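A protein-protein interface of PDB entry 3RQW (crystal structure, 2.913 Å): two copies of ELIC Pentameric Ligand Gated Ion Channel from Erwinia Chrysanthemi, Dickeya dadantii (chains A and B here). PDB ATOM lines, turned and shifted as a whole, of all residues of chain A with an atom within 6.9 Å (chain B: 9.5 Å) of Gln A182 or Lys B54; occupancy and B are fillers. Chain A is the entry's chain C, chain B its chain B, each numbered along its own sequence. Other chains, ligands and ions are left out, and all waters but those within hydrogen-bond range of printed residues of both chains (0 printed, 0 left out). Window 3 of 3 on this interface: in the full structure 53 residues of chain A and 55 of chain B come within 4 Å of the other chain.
The side-chain hydroxyl (OG1) of Thr B50 lies within hydrogen-bond range of the backbone carbonyl oxygen (O) of Lys B54, 2.6 Å away. The backbone carbonyl oxygen (O) of Gln A185 lies within hydrogen-bond range of the side-chain hydroxyl (OG) of Ser A180 (2.7 Å). OG of Ser A180 lies within hydrogen-bond range of O of Gln A182 (3.0 Å).
O of Ser A180 touches CZ of Phe B95, at 3.7 Å. Pro B55 touches Val A181. Phe B95 touches Val A181 (CE1 to O, 3.8 Å). Lys B54 touches Gln A182.
Gln A182 touches just one residue of chain B: Lys B54. Lys B54 touches one residue of chain A. Ser A180 touches one residue of chain B. Of the printed residues of chain B, Val A181 touches Pro B55 and Phe B95. No residue of chain B comes within 4 Å of Pro A183. No residue of chain B comes within 4 Å of Gln A185. Of the printed residues of chain A, Pro B55 touches Val A181 (3.4 Å). Of the printed residues of chain A, Phe B95 touches Ser A180 and Val A181. Met B93 touches none of the printed residues of chain A. The nearest residue of chain B that does not touch Gln A182 is Pro B55 (4.3 Å). The nearest residue of chain A that does not touch Lys B54 is Val A181 (4.9 Å).
Of the 10 printed residues of chain A, 3 touch a printed residue of chain B. Hydrophobic or aromatic side chains of chain A within 4 Å of the printed part of chain B: Val A181. Hydrophobic or aromatic side chains of chain B within 4 Å of the printed part of chain A: Pro B55 and Phe B95.
No position is printed for both chains. Of the 4 pairs that touch across the chains among the printed residues, none has its exchanged pair printed and touching as well.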
ATOM      1  N   ASN A 136      26.103 -28.814 -13.485  1.00  0.00           N
ATOM      2  CA  ASN A 136      25.086 -29.167 -14.463  1.00  0.00           C
ATOM      3  C   ASN A 136      24.947 -28.001 -15.417  1.00  0.00           C
ATOM      4  O   ASN A 136      24.611 -28.195 -16.577  1.00  0.00           O
ATOM      5  CB  ASN A 136      23.749 -29.413 -13.791  1.00  0.00           C
ATOM      6  CG  ASN A 136      23.220 -28.167 -13.062  1.00  0.00           C
ATOM      7  OD1 ASN A 136      22.737 -27.212 -13.698  1.00  0.00           O
ATOM      8  ND2 ASN A 136      23.311 -28.174 -11.721  1.00  0.00           N
ATOM      9  N   ASN A 137      25.234 -26.800 -14.894  1.00  0.00           N
ATOM     10  CA  ASN A 137      25.035 -25.489 -15.560  1.00  0.00           C
ATOM     11  C   ASN A 137      26.184 -25.052 -16.479  1.00  0.00           C
ATOM     12  O   ASN A 137      26.589 -23.879 -16.510  1.00  0.00           O
ATOM     13  CB  ASN A 137      24.715 -24.393 -14.521  1.00  0.00           C
ATOM     14  CG  ASN A 137      25.699 -24.377 -13.321  1.00  0.00           C
ATOM     15  OD1 ASN A 137      25.563 -25.139 -12.347  1.00  0.00           O
ATOM     16  ND2 ASN A 137      26.671 -23.476 -13.385  1.00  0.00           N
ATOM     17  N   SER A 179      20.805 -33.386  -5.388  1.00  0.00           N
ATOM     18  CA  SER A 179      20.423 -31.981  -5.250  1.00  0.00           C
ATOM     19  C   SER A 179      21.331 -31.090  -6.095  1.00  0.00           C
ATOM     20  O   SER A 179      22.543 -31.323  -6.189  1.00  0.00           O
ATOM     21  CB  SER A 179      20.468 -31.538  -3.784  1.00  0.00           C
ATOM     22  OG  SER A 179      19.707 -32.398  -2.948  1.00  0.00           O
ATOM     23  N   SER A 180      20.745 -30.073  -6.712  1.00  0.00           N
ATOM     24  CA  SER A 180      21.510 -29.188  -7.584  1.00  0.00           C
ATOM     25  C   SER A 180      21.406 -27.710  -7.198  1.00  0.00           C
ATOM     26  O   SER A 180      20.691 -27.346  -6.276  1.00  0.00           O
ATOM     27  CB  SER A 180      21.116 -29.403  -9.053  1.00  0.00           C
ATOM     28  OG  SER A 180      19.709 -29.409  -9.209  1.00  0.00           O
ATOM     29  N   VAL A 181      22.147 -26.869  -7.906  1.00  0.00           N
ATOM     30  CA  VAL A 181      22.140 -25.432  -7.668  1.00  0.00           C
ATOM     31  C   VAL A 181      20.714 -24.859  -7.599  1.00  0.00           C
ATOM     32  O   VAL A 181      20.332 -24.254  -6.595  1.00  0.00           O
ATOM     33  CB  VAL A 181      22.987 -24.697  -8.740  1.00  0.00           C
ATOM     34  CG1 VAL A 181      22.664 -23.205  -8.775  1.00  0.00           C
ATOM     35  CG2 VAL A 181      24.454 -24.907  -8.467  1.00  0.00           C
ATOM     36  N   GLN A 182      19.939 -25.050  -8.666  1.00  0.00           N
ATOM     37  CA  GLN A 182      18.542 -24.620  -8.704  1.00  0.00           C
ATOM     38  C   GLN A 182      17.635 -25.842  -8.575  1.00  0.00           C
ATOM     39  O   GLN A 182      18.088 -26.967  -8.761  1.00  0.00           O
ATOM     40  CB  GLN A 182      18.233 -23.846  -9.994  1.00  0.00           C
ATOM     41  CG  GLN A 182      19.114 -22.618 -10.240  1.00  0.00           C
ATOM     42  CD  GLN A 182      19.075 -21.616  -9.103  1.00  0.00           C
ATOM     43  OE1 GLN A 182      18.095 -21.530  -8.359  1.00  0.00           O
ATOM     44  NE2 GLN A 182      20.153 -20.854  -8.958  1.00  0.00           N
ATOM     45  N   PRO A 183      16.346 -25.625  -8.261  1.00  0.00           N
ATOM     46  CA  PRO A 183      15.445 -26.746  -7.959  1.00  0.00           C
ATOM     47  C   PRO A 183      15.049 -27.563  -9.190  1.00  0.00           C
ATOM     48  O   PRO A 183      14.747 -28.751  -9.076  1.00  0.00           O
ATOM     49  CB  PRO A 183      14.219 -26.048  -7.379  1.00  0.00           C
ATOM     50  CG  PRO A 183      14.207 -24.715  -8.068  1.00  0.00           C
ATOM     51  CD  PRO A 183      15.648 -24.326  -8.208  1.00  0.00           C
ATOM     52  N   ASN A 184      15.051 -26.928 -10.353  1.00  0.00           N
ATOM     53  CA  ASN A 184      14.632 -27.593 -11.580  1.00  0.00           C
ATOM     54  C   ASN A 184      15.746 -28.392 -12.262  1.00  0.00           C
ATOM     55  O   ASN A 184      15.521 -29.517 -12.715  1.00  0.00           O
ATOM     56  CB  ASN A 184      14.060 -26.556 -12.554  1.00  0.00           C
ATOM     57  CG  ASN A 184      13.723 -27.150 -13.915  1.00  0.00           C
ATOM     58  OD1 ASN A 184      13.357 -28.324 -14.022  1.00  0.00           O
ATOM     59  ND2 ASN A 184      13.851 -26.338 -14.963  1.00  0.00           N
ATOM     60  N   GLN A 185      16.942 -27.805 -12.307  1.00  0.00           N
ATOM     61  CA  GLN A 185      18.033 -28.256 -13.177  1.00  0.00           C
ATOM     62  C   GLN A 185      18.919 -29.387 -12.631  1.00  0.00           C
ATOM     63  O   GLN A 185      19.848 -29.148 -11.863  1.00  0.00           O
ATOM     64  CB  GLN A 185      18.894 -27.055 -13.582  1.00  0.00           C
ATOM     65  CG  GLN A 185      19.264 -26.129 -12.436  1.00  0.00           C
ATOM     66  CD  GLN A 185      19.929 -24.843 -12.916  1.00  0.00           C
ATOM     67  OE1 GLN A 185      19.489 -24.234 -13.891  1.00  0.00           O
ATOM     68  NE2 GLN A 185      21.000 -24.433 -12.237  1.00  0.00           N
ATOM     69  N   ASN A 186      18.637 -30.615 -13.061  1.00  0.00           N
ATOM     70  CA  ASN A 186      19.405 -31.777 -12.623  1.00  0.00           C
ATOM     71  C   ASN A 186      19.918 -32.653 -13.784  1.00  0.00           C
ATOM     72  O   ASN A 186      19.906 -33.884 -13.721  1.00  0.00           O
ATOM     73  CB  ASN A 186      18.591 -32.600 -11.623  1.00  0.00           C
ATOM     74  CG  ASN A 186      17.185 -32.904 -12.119  1.00  0.00           C
ATOM     75  OD1 ASN A 186      16.884 -32.767 -13.306  1.00  0.00           O
ATOM     76  ND2 ASN A 186      16.316 -33.324 -11.205  1.00  0.00           N
ATOM     77  N   ARG B  48      24.770 -17.925   4.892  1.00  0.00           N
ATOM     78  CA  ARG B  48      26.020 -17.386   4.371  1.00  0.00           C
ATOM     79  C   ARG B  48      25.788 -16.454   3.185  1.00  0.00           C
ATOM     80  O   ARG B  48      24.815 -16.599   2.431  1.00  0.00           O
ATOM     81  CB  ARG B  48      26.930 -18.551   3.957  1.00  0.00           C
ATOM     82  CG  ARG B  48      28.211 -18.180   3.192  1.00  0.00           C
ATOM     83  CD  ARG B  48      29.077 -19.422   2.885  1.00  0.00           C
ATOM     84  NE  ARG B  48      29.459 -20.150   4.100  1.00  0.00           N
ATOM     85  CZ  ARG B  48      28.822 -21.224   4.578  1.00  0.00           C
ATOM     86  NH1 ARG B  48      27.764 -21.729   3.937  1.00  0.00           N
ATOM     87  NH2 ARG B  48      29.249 -21.808   5.701  1.00  0.00           N
ATOM     88  N   LYS B  49      26.685 -15.490   3.019  1.00  0.00           N
ATOM     89  CA  LYS B  49      26.637 -14.648   1.837  1.00  0.00           C
ATOM     90  C   LYS B  49      27.393 -15.341   0.704  1.00  0.00           C
ATOM     91  O   LYS B  49      28.552 -15.728   0.858  1.00  0.00           O
ATOM     92  CB  LYS B  49      27.223 -13.261   2.131  1.00  0.00           C
ATOM     93  CG  LYS B  49      27.205 -12.305   0.938  1.00  0.00           C
ATOM     94  CD  LYS B  49      25.794 -12.138   0.360  1.00  0.00           C
ATOM     95  CE  LYS B  49      25.782 -11.210  -0.861  1.00  0.00           C
ATOM     96  NZ  LYS B  49      24.423 -11.068  -1.483  1.00  0.00           N
ATOM     97  N   THR B  50      26.720 -15.521  -0.425  1.00  0.00           N
ATOM     98  CA  THR B  50      27.343 -16.138  -1.584  1.00  0.00           C
ATOM     99  C   THR B  50      27.194 -15.218  -2.794  1.00  0.00           C
ATOM    100  O   THR B  50      26.158 -14.581  -2.962  1.00  0.00           O
ATOM    101  CB  THR B  50      26.715 -17.521  -1.900  1.00  0.00           C
ATOM    102  OG1 THR B  50      25.405 -17.346  -2.452  1.00  0.00           O
ATOM    103  CG2 THR B  50      26.624 -18.377  -0.643  1.00  0.00           C
ATOM    104  N   PRO B  51      28.229 -15.149  -3.641  1.00  0.00           N
ATOM    105  CA  PRO B  51      28.174 -14.362  -4.877  1.00  0.00           C
ATOM    106  C   PRO B  51      26.825 -14.521  -5.569  1.00  0.00           C
ATOM    107  O   PRO B  51      26.298 -15.637  -5.621  1.00  0.00           O
ATOM    108  CB  PRO B  51      29.283 -14.983  -5.722  1.00  0.00           C
ATOM    109  CG  PRO B  51      30.284 -15.448  -4.712  1.00  0.00           C
ATOM    110  CD  PRO B  51      29.494 -15.895  -3.512  1.00  0.00           C
ATOM    111  N   GLY B  52      26.282 -13.427  -6.100  1.00  0.00           N
ATOM    112  CA  GLY B  52      24.890 -13.399  -6.517  1.00  0.00           C
ATOM    113  C   GLY B  52      24.087 -13.743  -5.280  1.00  0.00           C
ATOM    114  O   GLY B  52      24.271 -13.144  -4.222  1.00  0.00           O
ATOM    115  N   ASP B  53      23.195 -14.712  -5.396  1.00  0.00           N
ATOM    116  CA  ASP B  53      22.654 -15.350  -4.209  1.00  0.00           C
ATOM    117  C   ASP B  53      22.427 -16.786  -4.599  1.00  0.00           C
ATOM    118  O   ASP B  53      21.606 -17.499  -4.010  1.00  0.00           O
ATOM    119  CB  ASP B  53      21.364 -14.691  -3.724  1.00  0.00           C
ATOM    120  CG  ASP B  53      21.285 -14.632  -2.206  1.00  0.00           C
ATOM    121  OD1 ASP B  53      20.178 -14.823  -1.645  1.00  0.00           O
ATOM    122  OD2 ASP B  53      22.344 -14.398  -1.577  1.00  0.00           O
ATOM    123  N   LYS B  54      23.171 -17.183  -5.626  1.00  0.00           N
ATOM    124  CA  LYS B  54      23.198 -18.552  -6.096  1.00  0.00           C
ATOM    125  C   LYS B  54      24.063 -19.329  -5.126  1.00  0.00           C
ATOM    126  O   LYS B  54      24.980 -18.770  -4.526  1.00  0.00           O
ATOM    127  CB  LYS B  54      23.807 -18.600  -7.497  1.00  0.00           C
ATOM    128  CG  LYS B  54      23.272 -17.533  -8.453  1.00  0.00           C
ATOM    129  CD  LYS B  54      21.791 -17.743  -8.753  1.00  0.00           C
ATOM    130  CE  LYS B  54      21.288 -16.774  -9.811  1.00  0.00           C
ATOM    131  NZ  LYS B  54      19.846 -17.002 -10.116  1.00  0.00           N
ATOM    132  N   PRO B  55      23.768 -20.617  -4.951  1.00  0.00           N
ATOM    133  CA  PRO B  55      24.687 -21.420  -4.142  1.00  0.00           C
ATOM    134  C   PRO B  55      26.076 -21.456  -4.798  1.00  0.00           C
ATOM    135  O   PRO B  55      26.223 -21.287  -6.026  1.00  0.00           O
ATOM    136  CB  PRO B  55      24.028 -22.802  -4.114  1.00  0.00           C
ATOM    137  CG  PRO B  55      23.087 -22.821  -5.274  1.00  0.00           C
ATOM    138  CD  PRO B  55      22.665 -21.405  -5.520  1.00  0.00           C
ATOM    139  N   LEU B  56      27.092 -21.644  -3.962  1.00  0.00           N
ATOM    140  CA  LEU B  56      28.479 -21.578  -4.394  1.00  0.00           C
ATOM    141  C   LEU B  56      29.106 -22.967  -4.486  1.00  0.00           C
ATOM    142  O   LEU B  56      28.918 -23.811  -3.596  1.00  0.00           O
ATOM    143  CB  LEU B  56      29.271 -20.734  -3.409  1.00  0.00           C
ATOM    144  CG  LEU B  56      30.751 -20.621  -3.734  1.00  0.00           C
ATOM    145  CD1 LEU B  56      30.947 -20.095  -5.160  1.00  0.00           C
ATOM    146  CD2 LEU B  56      31.450 -19.746  -2.707  1.00  0.00           C
ATOM    147  N   ILE B  57      29.851 -23.205  -5.561  1.00  0.00           N
ATOM    148  CA  ILE B  57      30.547 -24.483  -5.724  1.00  0.00           C
ATOM    149  C   ILE B  57      32.060 -24.388  -5.462  1.00  0.00           C
ATOM    150  O   ILE B  57      32.735 -23.463  -5.911  1.00  0.00           O
ATOM    151  CB  ILE B  57      30.275 -25.073  -7.101  1.00  0.00           C
ATOM    152  CG1 ILE B  57      28.948 -25.832  -7.074  1.00  0.00           C
ATOM    153  CG2 ILE B  57      31.418 -25.967  -7.526  1.00  0.00           C
ATOM    154  CD1 ILE B  57      28.352 -26.048  -8.464  1.00  0.00           C
ATOM    155  N   TRP B  66      38.883 -23.138   2.290  1.00  0.00           N
ATOM    156  CA  TRP B  66      37.706 -22.789   3.060  1.00  0.00           C
ATOM    157  C   TRP B  66      37.772 -23.325   4.481  1.00  0.00           C
ATOM    158  O   TRP B  66      37.263 -22.711   5.413  1.00  0.00           O
ATOM    159  CB  TRP B  66      36.448 -23.300   2.371  1.00  0.00           C
ATOM    160  CG  TRP B  66      36.041 -22.451   1.236  1.00  0.00           C
ATOM    161  CD1 TRP B  66      36.680 -22.315   0.041  1.00  0.00           C
ATOM    162  CD2 TRP B  66      34.903 -21.598   1.184  1.00  0.00           C
ATOM    163  NE1 TRP B  66      36.004 -21.426  -0.763  1.00  0.00           N
ATOM    164  CE2 TRP B  66      34.909 -20.971  -0.081  1.00  0.00           C
ATOM    165  CE3 TRP B  66      33.884 -21.292   2.087  1.00  0.00           C
ATOM    166  CZ2 TRP B  66      33.935 -20.063  -0.465  1.00  0.00           C
ATOM    167  CZ3 TRP B  66      32.918 -20.394   1.705  1.00  0.00           C
ATOM    168  CH2 TRP B  66      32.946 -19.789   0.439  1.00  0.00           C
ATOM    169  N   MET B  93      29.107 -27.969  -2.124  1.00  0.00           N
ATOM    170  CA  MET B  93      28.088 -27.042  -2.609  1.00  0.00           C
ATOM    171  C   MET B  93      27.580 -26.248  -1.401  1.00  0.00           C
ATOM    172  O   MET B  93      27.050 -26.815  -0.436  1.00  0.00           O
ATOM    173  CB  MET B  93      26.963 -27.808  -3.295  1.00  0.00           C
ATOM    174  CG  MET B  93      26.000 -26.961  -4.080  1.00  0.00           C
ATOM    175  SD  MET B  93      24.908 -28.029  -5.033  1.00  0.00           S
ATOM    176  CE  MET B  93      25.992 -28.514  -6.365  1.00  0.00           C
ATOM    177  N   LEU B  94      27.805 -24.941  -1.434  1.00  0.00           N
ATOM    178  CA  LEU B  94      27.444 -24.069  -0.328  1.00  0.00           C
ATOM    179  C   LEU B  94      26.224 -23.233  -0.675  1.00  0.00           C
ATOM    180  O   LEU B  94      26.307 -22.316  -1.508  1.00  0.00           O
ATOM    181  CB  LEU B  94      28.602 -23.136   0.015  1.00  0.00           C
ATOM    182  CG  LEU B  94      29.892 -23.816   0.441  1.00  0.00           C
ATOM    183  CD1 LEU B  94      30.926 -22.775   0.858  1.00  0.00           C
ATOM    184  CD2 LEU B  94      29.629 -24.819   1.555  1.00  0.00           C
ATOM    185  N   PHE B  95      25.095 -23.549  -0.039  1.00  0.00           N
ATOM    186  CA  PHE B  95      23.881 -22.741  -0.183  1.00  0.00           C
ATOM    187  C   PHE B  95      23.895 -21.563   0.779  1.00  0.00           C
ATOM    188  O   PHE B  95      24.465 -21.673   1.872  1.00  0.00           O
ATOM    189  CB  PHE B  95      22.635 -23.584   0.050  1.00  0.00           C
ATOM    190  CG  PHE B  95      22.421 -24.610  -0.994  1.00  0.00           C
ATOM    191  CD1 PHE B  95      21.761 -24.291  -2.166  1.00  0.00           C
ATOM    192  CD2 PHE B  95      22.907 -25.889  -0.827  1.00  0.00           C
ATOM    193  CE1 PHE B  95      21.567 -25.235  -3.144  1.00  0.00           C
ATOM    194  CE2 PHE B  95      22.718 -26.843  -1.801  1.00  0.00           C
ATOM    195  CZ  PHE B  95      22.043 -26.515  -2.962  1.00  0.00           C
ATOM    196  N   PRO B  96      23.266 -20.439   0.372  1.00  0.00           N
ATOM    197  CA  PRO B  96      23.236 -19.180   1.133  1.00  0.00           C
ATOM    198  C   PRO B  96      22.355 -19.294   2.385  1.00  0.00           C
ATOM    199  O   PRO B  96      22.591 -18.621   3.397  1.00  0.00           O
ATOM    200  CB  PRO B  96      22.625 -18.191   0.140  1.00  0.00           C
ATOM    201  CG  PRO B  96      21.735 -19.041  -0.713  1.00  0.00           C
ATOM    202  CD  PRO B  96      22.446 -20.360  -0.854  1.00  0.00           C
ATOM    203  N   ASP B  97      21.348 -20.157   2.311  1.00  0.00           N
ATOM    204  CA  ASP B  97      20.544 -20.472   3.471  1.00  0.00           C
ATOM    205  C   ASP B  97      21.211 -21.436   4.456  1.00  0.00           C
ATOM    206  O   ASP B  97      20.591 -21.850   5.427  1.00  0.00           O
ATOM    207  CB  ASP B  97      19.200 -21.029   3.025  1.00  0.00           C
ATOM    208  CG  ASP B  97      19.334 -22.294   2.224  1.00  0.00           C
ATOM    209  OD1 ASP B  97      19.329 -23.376   2.851  1.00  0.00           O
ATOM    210  OD2 ASP B  97      19.430 -22.199   0.976  1.00  0.00           O
ATOM    211  N   ARG B  99      22.713 -24.549   3.821  1.00  0.00           N
ATOM    212  CA  ARG B  99      22.917 -25.934   3.412  1.00  0.00           C
ATOM    213  C   ARG B  99      24.364 -26.124   2.945  1.00  0.00           C
ATOM    214  O   ARG B  99      24.969 -25.232   2.328  1.00  0.00           O
ATOM    215  CB  ARG B  99      21.944 -26.352   2.306  1.00  0.00           C
ATOM    216  CG  ARG B  99      20.481 -26.323   2.701  1.00  0.00           C
ATOM    217  CD  ARG B  99      19.709 -27.488   2.099  1.00  0.00           C
ATOM    218  NE  ARG B  99      19.401 -27.400   0.665  1.00  0.00           N
ATOM    219  CZ  ARG B  99      19.088 -26.287   0.003  1.00  0.00           C
ATOM    220  NH1 ARG B  99      19.046 -25.112   0.617  1.00  0.00           N
ATOM    221  NH2 ARG B  99      18.818 -26.355  -1.295  1.00  0.00           N
